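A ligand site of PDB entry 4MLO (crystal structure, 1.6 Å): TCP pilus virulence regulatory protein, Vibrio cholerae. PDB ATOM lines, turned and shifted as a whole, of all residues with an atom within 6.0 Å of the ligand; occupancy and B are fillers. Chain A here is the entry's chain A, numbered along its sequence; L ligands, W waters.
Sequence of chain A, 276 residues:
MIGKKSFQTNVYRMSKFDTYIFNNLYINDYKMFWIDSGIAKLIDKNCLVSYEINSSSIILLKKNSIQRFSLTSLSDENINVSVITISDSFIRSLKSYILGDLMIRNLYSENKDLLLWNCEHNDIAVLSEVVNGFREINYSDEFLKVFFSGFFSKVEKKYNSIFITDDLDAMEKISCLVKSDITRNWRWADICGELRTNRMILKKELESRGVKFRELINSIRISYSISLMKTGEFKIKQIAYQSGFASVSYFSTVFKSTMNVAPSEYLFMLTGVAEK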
ATOM      1  N   GLN A   8      -7.827  -0.859 -27.278  1.00  0.00           N
ATOM      2  CA  GLN A   8      -7.088  -2.096 -27.420  1.00  0.00           C
ATOM      3  C   GLN A   8      -6.225  -2.262 -26.168  1.00  0.00           C
ATOM      4  O   GLN A   8      -5.506  -1.332 -25.779  1.00  0.00           O
ATOM      5  CB  GLN A   8      -6.218  -2.056 -28.678  1.00  0.00           C
ATOM      6  CG  GLN A   8      -5.665  -3.392 -29.138  1.00  0.00           C
ATOM      7  CD  GLN A   8      -4.455  -3.826 -28.342  1.00  0.00           C
ATOM      8  OE1 GLN A   8      -3.680  -2.994 -27.879  1.00  0.00           O
ATOM      9  NE2 GLN A   8      -4.288  -5.122 -28.178  1.00  0.00           N
ATOM     10  N   ASN A  10      -3.663  -4.678 -23.482  1.00  0.00           N
ATOM     11  CA  ASN A  10      -2.698  -5.752 -23.321  1.00  0.00           C
ATOM     12  C   ASN A  10      -2.245  -5.755 -21.885  1.00  0.00           C
ATOM     13  O   ASN A  10      -2.134  -4.708 -21.246  1.00  0.00           O
ATOM     14  CB  ASN A  10      -1.486  -5.604 -24.259  1.00  0.00           C
ATOM     15  CG  ASN A  10      -1.831  -5.760 -25.696  1.00  0.00           C
ATOM     16  OD1 ASN A  10      -2.121  -4.780 -26.384  1.00  0.00           O
ATOM     17  ND2 ASN A  10      -1.841  -6.993 -26.173  1.00  0.00           N
ATOM     18  N   TYR A  12       0.969  -7.340 -19.777  1.00  0.00           N
ATOM     19  CA  TYR A  12       2.274  -7.968 -19.865  1.00  0.00           C
ATOM     20  C   TYR A  12       2.732  -8.437 -18.495  1.00  0.00           C
ATOM     21  O   TYR A  12       2.648  -7.694 -17.520  1.00  0.00           O
ATOM     22  CB  TYR A  12       3.301  -6.999 -20.418  1.00  0.00           C
ATOM     23  CG  TYR A  12       2.983  -6.557 -21.832  1.00  0.00           C
ATOM     24  CD1 TYR A  12       2.458  -5.293 -22.088  1.00  0.00           C
ATOM     25  CD2 TYR A  12       3.174  -7.407 -22.863  1.00  0.00           C
ATOM     26  CE1 TYR A  12       2.179  -4.905 -23.399  1.00  0.00           C
ATOM     27  CE2 TYR A  12       2.908  -7.017 -24.180  1.00  0.00           C
ATOM     28  CZ  TYR A  12       2.400  -5.785 -24.442  1.00  0.00           C
ATOM     29  OH  TYR A  12       2.152  -5.457 -25.773  1.00  0.00           O
ATOM     30  N   TYR A  20      12.496  -3.628 -18.700  1.00  0.00           N
ATOM     31  CA  TYR A  20      12.171  -3.415 -20.098  1.00  0.00           C
ATOM     32  C   TYR A  20      12.790  -2.101 -20.526  1.00  0.00           C
ATOM     33  O   TYR A  20      12.673  -1.098 -19.818  1.00  0.00           O
ATOM     34  CB  TYR A  20      10.666  -3.372 -20.306  1.00  0.00           C
ATOM     35  CG  TYR A  20       9.942  -4.676 -20.001  1.00  0.00           C
ATOM     36  CD1 TYR A  20       8.700  -4.668 -19.353  1.00  0.00           C
ATOM     37  CD2 TYR A  20      10.481  -5.891 -20.367  1.00  0.00           C
ATOM     38  CE1 TYR A  20       8.032  -5.853 -19.075  1.00  0.00           C
ATOM     39  CE2 TYR A  20       9.815  -7.094 -20.076  1.00  0.00           C
ATOM     40  CZ  TYR A  20       8.586  -7.055 -19.440  1.00  0.00           C
ATOM     41  OH  TYR A  20       7.922  -8.229 -19.169  1.00  0.00           O
ATOM     42  N   PHE A  22      13.209   0.543 -23.893  1.00  0.00           N
ATOM     43  CA  PHE A  22      12.722   0.959 -25.188  1.00  0.00           C
ATOM     44  C   PHE A  22      13.611   2.062 -25.745  1.00  0.00           C
ATOM     45  O   PHE A  22      13.915   3.024 -25.018  1.00  0.00           O
ATOM     46  CB  PHE A  22      11.293   1.454 -25.087  1.00  0.00           C
ATOM     47  CG  PHE A  22      10.374   0.452 -24.495  1.00  0.00           C
ATOM     48  CD1 PHE A  22       9.952  -0.631 -25.243  1.00  0.00           C
ATOM     49  CD2 PHE A  22      10.046   0.516 -23.154  1.00  0.00           C
ATOM     50  CE1 PHE A  22       9.129  -1.584 -24.684  1.00  0.00           C
ATOM     51  CE2 PHE A  22       9.232  -0.448 -22.594  1.00  0.00           C
ATOM     52  CZ  PHE A  22       8.773  -1.489 -23.359  1.00  0.00           C
ATOM     53  N   LEU A  25      11.128   4.051 -29.676  1.00  0.00           N
ATOM     54  CA  LEU A  25       9.782   3.457 -29.770  1.00  0.00           C
ATOM     55  C   LEU A  25       8.801   4.544 -30.238  1.00  0.00           C
ATOM     56  O   LEU A  25       8.523   5.478 -29.490  1.00  0.00           O
ATOM     57  CB  LEU A  25       9.341   2.894 -28.426  1.00  0.00           C
ATOM     58  CG  LEU A  25       7.975   2.202 -28.389  1.00  0.00           C
ATOM     59  CD1 LEU A  25       8.048   0.909 -29.200  1.00  0.00           C
ATOM     60  CD2 LEU A  25       7.466   1.990 -26.944  1.00  0.00           C
ATOM     61  N   ILE A  27       5.178   5.878 -30.969  1.00  0.00           N
ATOM     62  CA  ILE A  27       3.889   5.687 -30.316  1.00  0.00           C
ATOM     63  C   ILE A  27       2.844   5.937 -31.392  1.00  0.00           C
ATOM     64  O   ILE A  27       2.569   7.080 -31.755  1.00  0.00           O
ATOM     65  CB  ILE A  27       3.720   6.608 -29.111  1.00  0.00           C
ATOM     66  CG1 ILE A  27       4.845   6.370 -28.098  1.00  0.00           C
ATOM     67  CG2 ILE A  27       2.398   6.366 -28.476  1.00  0.00           C
ATOM     68  CD1 ILE A  27       4.974   4.926 -27.600  1.00  0.00           C
ATOM     69  N   LYS A  31      -1.396   6.133 -25.651  1.00  0.00           N
ATOM     70  CA  LYS A  31      -1.279   4.975 -24.763  1.00  0.00           C
ATOM     71  C   LYS A  31      -1.284   5.397 -23.305  1.00  0.00           C
ATOM     72  O   LYS A  31      -0.810   6.474 -22.943  1.00  0.00           O
ATOM     73  CB  LYS A  31       0.015   4.160 -25.034  1.00  0.00           C
ATOM     74  CG  LYS A  31      -0.085   3.342 -26.299  1.00  0.00           C
ATOM     75  CD  LYS A  31       1.167   2.575 -26.579  1.00  0.00           C
ATOM     76  CE  LYS A  31       1.144   2.043 -27.979  1.00  0.00           C
ATOM     77  NZ  LYS A  31       0.272   0.856 -28.062  1.00  0.00           N
ATOM     78  N   PHE A  33      -0.453   3.383 -19.427  1.00  0.00           N
ATOM     79  CA  PHE A  33      -0.098   2.120 -18.789  1.00  0.00           C
ATOM     80  C   PHE A  33       0.154   2.310 -17.303  1.00  0.00           C
ATOM     81  O   PHE A  33       0.370   3.426 -16.823  1.00  0.00           O
ATOM     82  CB  PHE A  33       1.100   1.430 -19.471  1.00  0.00           C
ATOM     83  CG  PHE A  33       2.437   2.092 -19.255  1.00  0.00           C
ATOM     84  CD1 PHE A  33       2.968   2.950 -20.207  1.00  0.00           C
ATOM     85  CD2 PHE A  33       3.206   1.792 -18.129  1.00  0.00           C
ATOM     86  CE1 PHE A  33       4.213   3.524 -20.031  1.00  0.00           C
ATOM     87  CE2 PHE A  33       4.468   2.362 -17.951  1.00  0.00           C
ATOM     88  CZ  PHE A  33       4.970   3.221 -18.899  1.00  0.00           C
ATOM     89  N   LEU A  61       1.427   8.217 -22.751  1.00  0.00           N
ATOM     90  CA  LEU A  61       2.395   8.408 -23.832  1.00  0.00           C
ATOM     91  C   LEU A  61       1.691   9.056 -25.015  1.00  0.00           C
ATOM     92  O   LEU A  61       0.652   8.578 -25.482  1.00  0.00           O
ATOM     93  CB  LEU A  61       3.043   7.086 -24.269  1.00  0.00           C
ATOM     94  CG  LEU A  61       3.750   6.270 -23.168  1.00  0.00           C
ATOM     95  CD1 LEU A  61       4.317   4.996 -23.768  1.00  0.00           C
ATOM     96  CD2 LEU A  61       4.841   7.080 -22.518  1.00  0.00           C
ATOM     97  N   PHE A  69      12.931   4.994 -22.815  1.00  0.00           N
ATOM     98  CA  PHE A  69      12.729   4.853 -21.381  1.00  0.00           C
ATOM     99  C   PHE A  69      12.891   3.403 -21.001  1.00  0.00           C
ATOM    100  O   PHE A  69      12.859   2.503 -21.849  1.00  0.00           O
ATOM    101  CB  PHE A  69      11.370   5.388 -20.911  1.00  0.00           C
ATOM    102  CG  PHE A  69      10.176   4.556 -21.329  1.00  0.00           C
ATOM    103  CD1 PHE A  69       9.526   4.827 -22.530  1.00  0.00           C
ATOM    104  CD2 PHE A  69       9.629   3.598 -20.494  1.00  0.00           C
ATOM    105  CE1 PHE A  69       8.413   4.123 -22.902  1.00  0.00           C
ATOM    106  CE2 PHE A  69       8.510   2.869 -20.854  1.00  0.00           C
ATOM    107  CZ  PHE A  69       7.885   3.143 -22.066  1.00  0.00           C
ATOM    108  N   LEU A  71      11.660   0.595 -17.731  1.00  0.00           N
ATOM    109  CA  LEU A  71      10.796   0.272 -16.600  1.00  0.00           C
ATOM    110  C   LEU A  71      11.414  -0.914 -15.878  1.00  0.00           C
ATOM    111  O   LEU A  71      11.563  -1.996 -16.457  1.00  0.00           O
ATOM    112  CB  LEU A  71       9.367  -0.027 -17.057  1.00  0.00           C
ATOM    113  CG  LEU A  71       8.355  -0.208 -15.916  1.00  0.00           C
ATOM    114  CD1 LEU A  71       8.163   1.099 -15.137  1.00  0.00           C
ATOM    115  CD2 LEU A  71       7.019  -0.732 -16.412  1.00  0.00           C
ATOM    116  N   VAL A  81       1.716  -5.447 -16.095  1.00  0.00           N
ATOM    117  CA  VAL A  81       1.649  -4.105 -16.660  1.00  0.00           C
ATOM    118  C   VAL A  81       0.500  -4.062 -17.651  1.00  0.00           C
ATOM    119  O   VAL A  81       0.518  -4.744 -18.681  1.00  0.00           O
ATOM    120  CB  VAL A  81       2.966  -3.705 -17.341  1.00  0.00           C
ATOM    121  CG1 VAL A  81       2.951  -2.223 -17.699  1.00  0.00           C
ATOM    122  CG2 VAL A  81       4.140  -4.012 -16.432  1.00  0.00           C
ATOM    123  N   VAL A  83      -1.723  -2.024 -20.434  1.00  0.00           N
ATOM    124  CA  VAL A  83      -1.493  -1.026 -21.469  1.00  0.00           C
ATOM    125  C   VAL A  83      -2.790  -0.826 -22.236  1.00  0.00           C
ATOM    126  O   VAL A  83      -3.285  -1.757 -22.874  1.00  0.00           O
ATOM    127  CB  VAL A  83      -0.381  -1.457 -22.430  1.00  0.00           C
ATOM    128  CG1 VAL A  83      -0.101  -0.347 -23.493  1.00  0.00           C
ATOM    129  CG2 VAL A  83       0.860  -1.788 -21.671  1.00  0.00           C
ATOM    130  N   THR A  85      -4.301   1.152 -25.434  1.00  0.00           N
ATOM    131  CA  THR A  85      -4.052   1.892 -26.665  1.00  0.00           C
ATOM    132  C   THR A  85      -5.392   2.410 -27.152  1.00  0.00           C
ATOM    133  O   THR A  85      -6.324   1.624 -27.346  1.00  0.00           O
ATOM    134  CB  THR A  85      -3.414   1.011 -27.740  1.00  0.00           C
ATOM    135  OG1 THR A  85      -2.197   0.418 -27.238  1.00  0.00           O
ATOM    136  CG2 THR A  85      -3.097   1.825 -28.969  1.00  0.00           C
ATOM    137  N   ILE A 226       4.367  -4.623 -34.472  1.00  0.00           N
ATOM    138  CA  ILE A 226       3.781  -4.898 -33.164  1.00  0.00           C
ATOM    139  C   ILE A 226       2.273  -4.989 -33.319  1.00  0.00           C
ATOM    140  O   ILE A 226       1.644  -5.932 -32.847  1.00  0.00           O
ATOM    141  CB  ILE A 226       4.217  -3.833 -32.152  1.00  0.00           C
ATOM    142  CG1 ILE A 226       5.668  -4.090 -31.769  1.00  0.00           C
ATOM    143  CG2 ILE A 226       3.392  -3.889 -30.904  1.00  0.00           C
ATOM    144  CD1 ILE A 226       6.315  -2.916 -31.083  1.00  0.00           C
ATOM    145  N   LYS A 230      -0.124  -8.180 -32.529  1.00  0.00           N
ATOM    146  CA  LYS A 230      -1.264  -8.108 -31.622  1.00  0.00           C
ATOM    147  C   LYS A 230      -2.549  -8.624 -32.262  1.00  0.00           C
ATOM    148  O   LYS A 230      -3.474  -8.964 -31.528  1.00  0.00           O
ATOM    149  CB  LYS A 230      -1.460  -6.671 -31.138  1.00  0.00           C
ATOM    150  CG  LYS A 230      -0.448  -6.219 -30.121  1.00  0.00           C
ATOM    151  CD  LYS A 230      -0.738  -4.777 -29.704  1.00  0.00           C
ATOM    152  CE  LYS A 230       0.189  -4.362 -28.610  1.00  0.00           C
ATOM    153  NZ  LYS A 230      -0.303  -3.095 -28.003  1.00  0.00           N
ATOM    154  N   MET A 259      13.150  -2.770 -28.849  1.00  0.00           N
ATOM    155  CA  MET A 259      12.434  -3.433 -27.775  1.00  0.00           C
ATOM    156  C   MET A 259      13.353  -4.166 -26.801  1.00  0.00           C
ATOM    157  O   MET A 259      12.870  -4.634 -25.757  1.00  0.00           O
ATOM    158  CB  MET A 259      11.440  -4.411 -28.370  1.00  0.00           C
ATOM    159  CG  MET A 259      10.453  -3.781 -29.353  1.00  0.00           C
ATOM    160  SD  MET A 259       9.235  -2.740 -28.502  1.00  0.00           S
ATOM    161  CE  MET A 259       8.151  -3.894 -27.752  1.00  0.00           C
ATOM    162  N   ASN A 260      14.641  -4.293 -27.127  1.00  0.00           N
ATOM    163  CA  ASN A 260      15.629  -5.032 -26.331  1.00  0.00           C
ATOM    164  C   ASN A 260      15.281  -6.516 -26.150  1.00  0.00           C
ATOM    165  O   ASN A 260      15.772  -7.156 -25.208  1.00  0.00           O
ATOM    166  CB  ASN A 260      15.808  -4.367 -24.977  1.00  0.00           C
ATOM    167  CG  ASN A 260      17.168  -4.598 -24.389  1.00  0.00           C
ATOM    168  OD1 ASN A 260      18.231  -4.386 -25.035  1.00  0.00           O
ATOM    169  ND2 ASN A 260      17.164  -5.001 -23.120  1.00  0.00           N
ATOM    170  N   VAL A 261      14.453  -7.077 -27.039  1.00  0.00           N
ATOM    171  CA  VAL A 261      14.144  -8.501 -27.080  1.00  0.00           C
ATOM    172  C   VAL A 261      13.969  -8.879 -28.541  1.00  0.00           C
ATOM    173  O   VAL A 261      13.788  -8.021 -29.406  1.00  0.00           O
ATOM    174  CB  VAL A 261      12.872  -8.890 -26.281  1.00  0.00           C
ATOM    175  CG1 VAL A 261      13.013  -8.458 -24.843  1.00  0.00           C
ATOM    176  CG2 VAL A 261      11.609  -8.278 -26.879  1.00  0.00           C
ATOM    177  N   TYR A 266       8.924 -11.281 -27.947  1.00  0.00           N
ATOM    178  CA  TYR A 266       7.740 -10.439 -27.786  1.00  0.00           C
ATOM    179  C   TYR A 266       6.477 -11.241 -28.090  1.00  0.00           C
ATOM    180  O   TYR A 266       5.470 -11.154 -27.368  1.00  0.00           O
ATOM    181  CB  TYR A 266       7.855  -9.190 -28.670  1.00  0.00           C
ATOM    182  CG  TYR A 266       6.616  -8.337 -28.592  1.00  0.00           C
ATOM    183  CD1 TYR A 266       5.720  -8.247 -29.664  1.00  0.00           C
ATOM    184  CD2 TYR A 266       6.307  -7.674 -27.413  1.00  0.00           C
ATOM    185  CE1 TYR A 266       4.576  -7.486 -29.544  1.00  0.00           C
ATOM    186  CE2 TYR A 266       5.159  -6.908 -27.300  1.00  0.00           C
ATOM    187  CZ  TYR A 266       4.294  -6.837 -28.362  1.00  0.00           C
ATOM    188  OH  TYR A 266       3.146  -6.100 -28.243  1.00  0.00           O
ATOM    189  N   MET A 269       5.554 -12.959 -25.141  1.00  0.00           N
ATOM    190  CA  MET A 269       4.946 -12.103 -24.129  1.00  0.00           C
ATOM    191  C   MET A 269       3.479 -11.855 -24.414  1.00  0.00           C
ATOM    192  O   MET A 269       2.679 -11.649 -23.492  1.00  0.00           O
ATOM    193  CB  MET A 269       5.700 -10.775 -24.054  1.00  0.00           C
ATOM    194  CG  MET A 269       7.140 -10.964 -23.656  1.00  0.00           C
ATOM    195  SD  MET A 269       8.021  -9.396 -23.656  1.00  0.00           S
ATOM    196  CE  MET A 269       7.355  -8.704 -22.134  1.00  0.00           C
HETATM  197  C1  LIG L   1       2.566  -2.136 -26.915  1.00  0.00           C
HETATM  198  O1  LIG L   1       1.746  -2.839 -26.271  1.00  0.00           O
HETATM  199  O2  LIG L   1       2.182  -1.272 -27.742  1.00  0.00           O
HETATM  200  C2  LIG L   1       4.041  -2.335 -26.734  1.00  0.00           C
HETATM  201  C3  LIG L   1       4.745  -1.047 -26.267  1.00  0.00           C
HETATM  202  C4  LIG L   1       4.160  -0.593 -24.935  1.00  0.00           C
HETATM  203  C5  LIG L   1       4.854   0.635 -24.371  1.00  0.00           C
HETATM  204  C6  LIG L   1       4.153   1.149 -23.119  1.00  0.00           C
HETATM  205  C7  LIG L   1       4.165   0.143 -21.968  1.00  0.00           C
HETATM  206  C8  LIG L   1       5.568  -0.041 -21.425  1.00  0.00           C
HETATM  207  C9  LIG L   1       5.621  -1.099 -20.322  1.00  0.00           C
HETATM  208  C10 LIG L   1       5.564  -2.416 -20.549  1.00  0.00           C
HETATM  209  C11 LIG L   1       5.394  -2.998 -21.943  1.00  0.00           C
HETATM  210  C12 LIG L   1       6.088  -4.357 -22.121  1.00  0.00           C
HETATM  211  C13 LIG L   1       6.158  -4.653 -23.620  1.00  0.00           C
HETATM  212  C14 LIG L   1       7.175  -5.698 -24.022  1.00  0.00           C
HETATM  213  C15 LIG L   1       8.591  -5.324 -23.585  1.00  0.00           C
HETATM  214  C16 LIG L   1       9.637  -5.975 -24.451  1.00  0.00           C
HETATM  215  O   HOH W   1       3.577  -0.192 -30.183  1.00  0.00           O
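NZ of Lys 230 lies within hydrogen-bond range of OD1 of Asn 10, at 3.0 Å.
NZ of Lys 230 lies within hydrogen-bond range of OE1 of Gln 8, 3.4 Å away.
The backbone NH of Val 81 sits at hydrogen-bond distance from the backbone carbonyl oxygen of Tyr 12.
The backbone carbonyl oxygen (O) of Lys 31 is in hydrogen-bond range of the backbone NH (N) of Leu 61, 2.8 Å away.
The side-chain hydroxyl of Thr 85 is in hydrogen-bond range of the side-chain amino group of Lys 31 (2.6 Å).
The backbone carbonyl oxygen of Tyr 20 lies within hydrogen-bond range of the backbone NH of Leu 71 (2.9 Å).
The backbone NH (N) of Val 83 lies within hydrogen-bond range of the backbone carbonyl oxygen (O) of Asn 10 (2.8 Å).
The backbone carbonyl oxygen (O) of Phe 69 is in hydrogen-bond range of the backbone NH (N) of Phe 22, at 2.9 Å.
The side-chain amino group of Lys 230 is in salt-bridge range of an oxygen (O1) of the ligand (2.7 Å).
An oxygen (O1) of the ligand is in hydrogen-bond range of the side-chain hydroxyl (OH) of Tyr 12.
The side-chain amino group of Lys 31 lies within salt-bridge range of an oxygen (O2) of the ligand (2.9 Å).
Tyr 20 touches the ligand (CD2 to C15, 3.8 Å).
CZ of Phe 22 touches C15 of the ligand (3.8 Å).
Leu 25 touches the ligand.
Phe 33 touches the ligand.
CD1 of Leu 61 touches C6 of the ligand, at 3.9 Å.
Phe 69 touches the ligand (CZ to C8, 3.99 Å).
Val 81 touches the ligand (CG1 to C10, 3.9 Å).
CG2 of Val 83 touches C7 of the ligand (3.8 Å).
Met 259 touches the ligand (O to C16, 3.7 Å).
CG2 of Val 261 touches C16 of the ligand, 3.9 Å away.
Met 269 touches the ligand (CE to C14, 3.6 Å).
Hydrophobic or aromatic side chains that line the ligand: Tyr 12, Tyr 20, Phe 22, Leu 25, Phe 33, Leu 61, Phe 69, Val 81, Val 83, Val 261 and Met 269.
Along chain A the residues within 4 Å of the ligand span positions 12 to 269.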
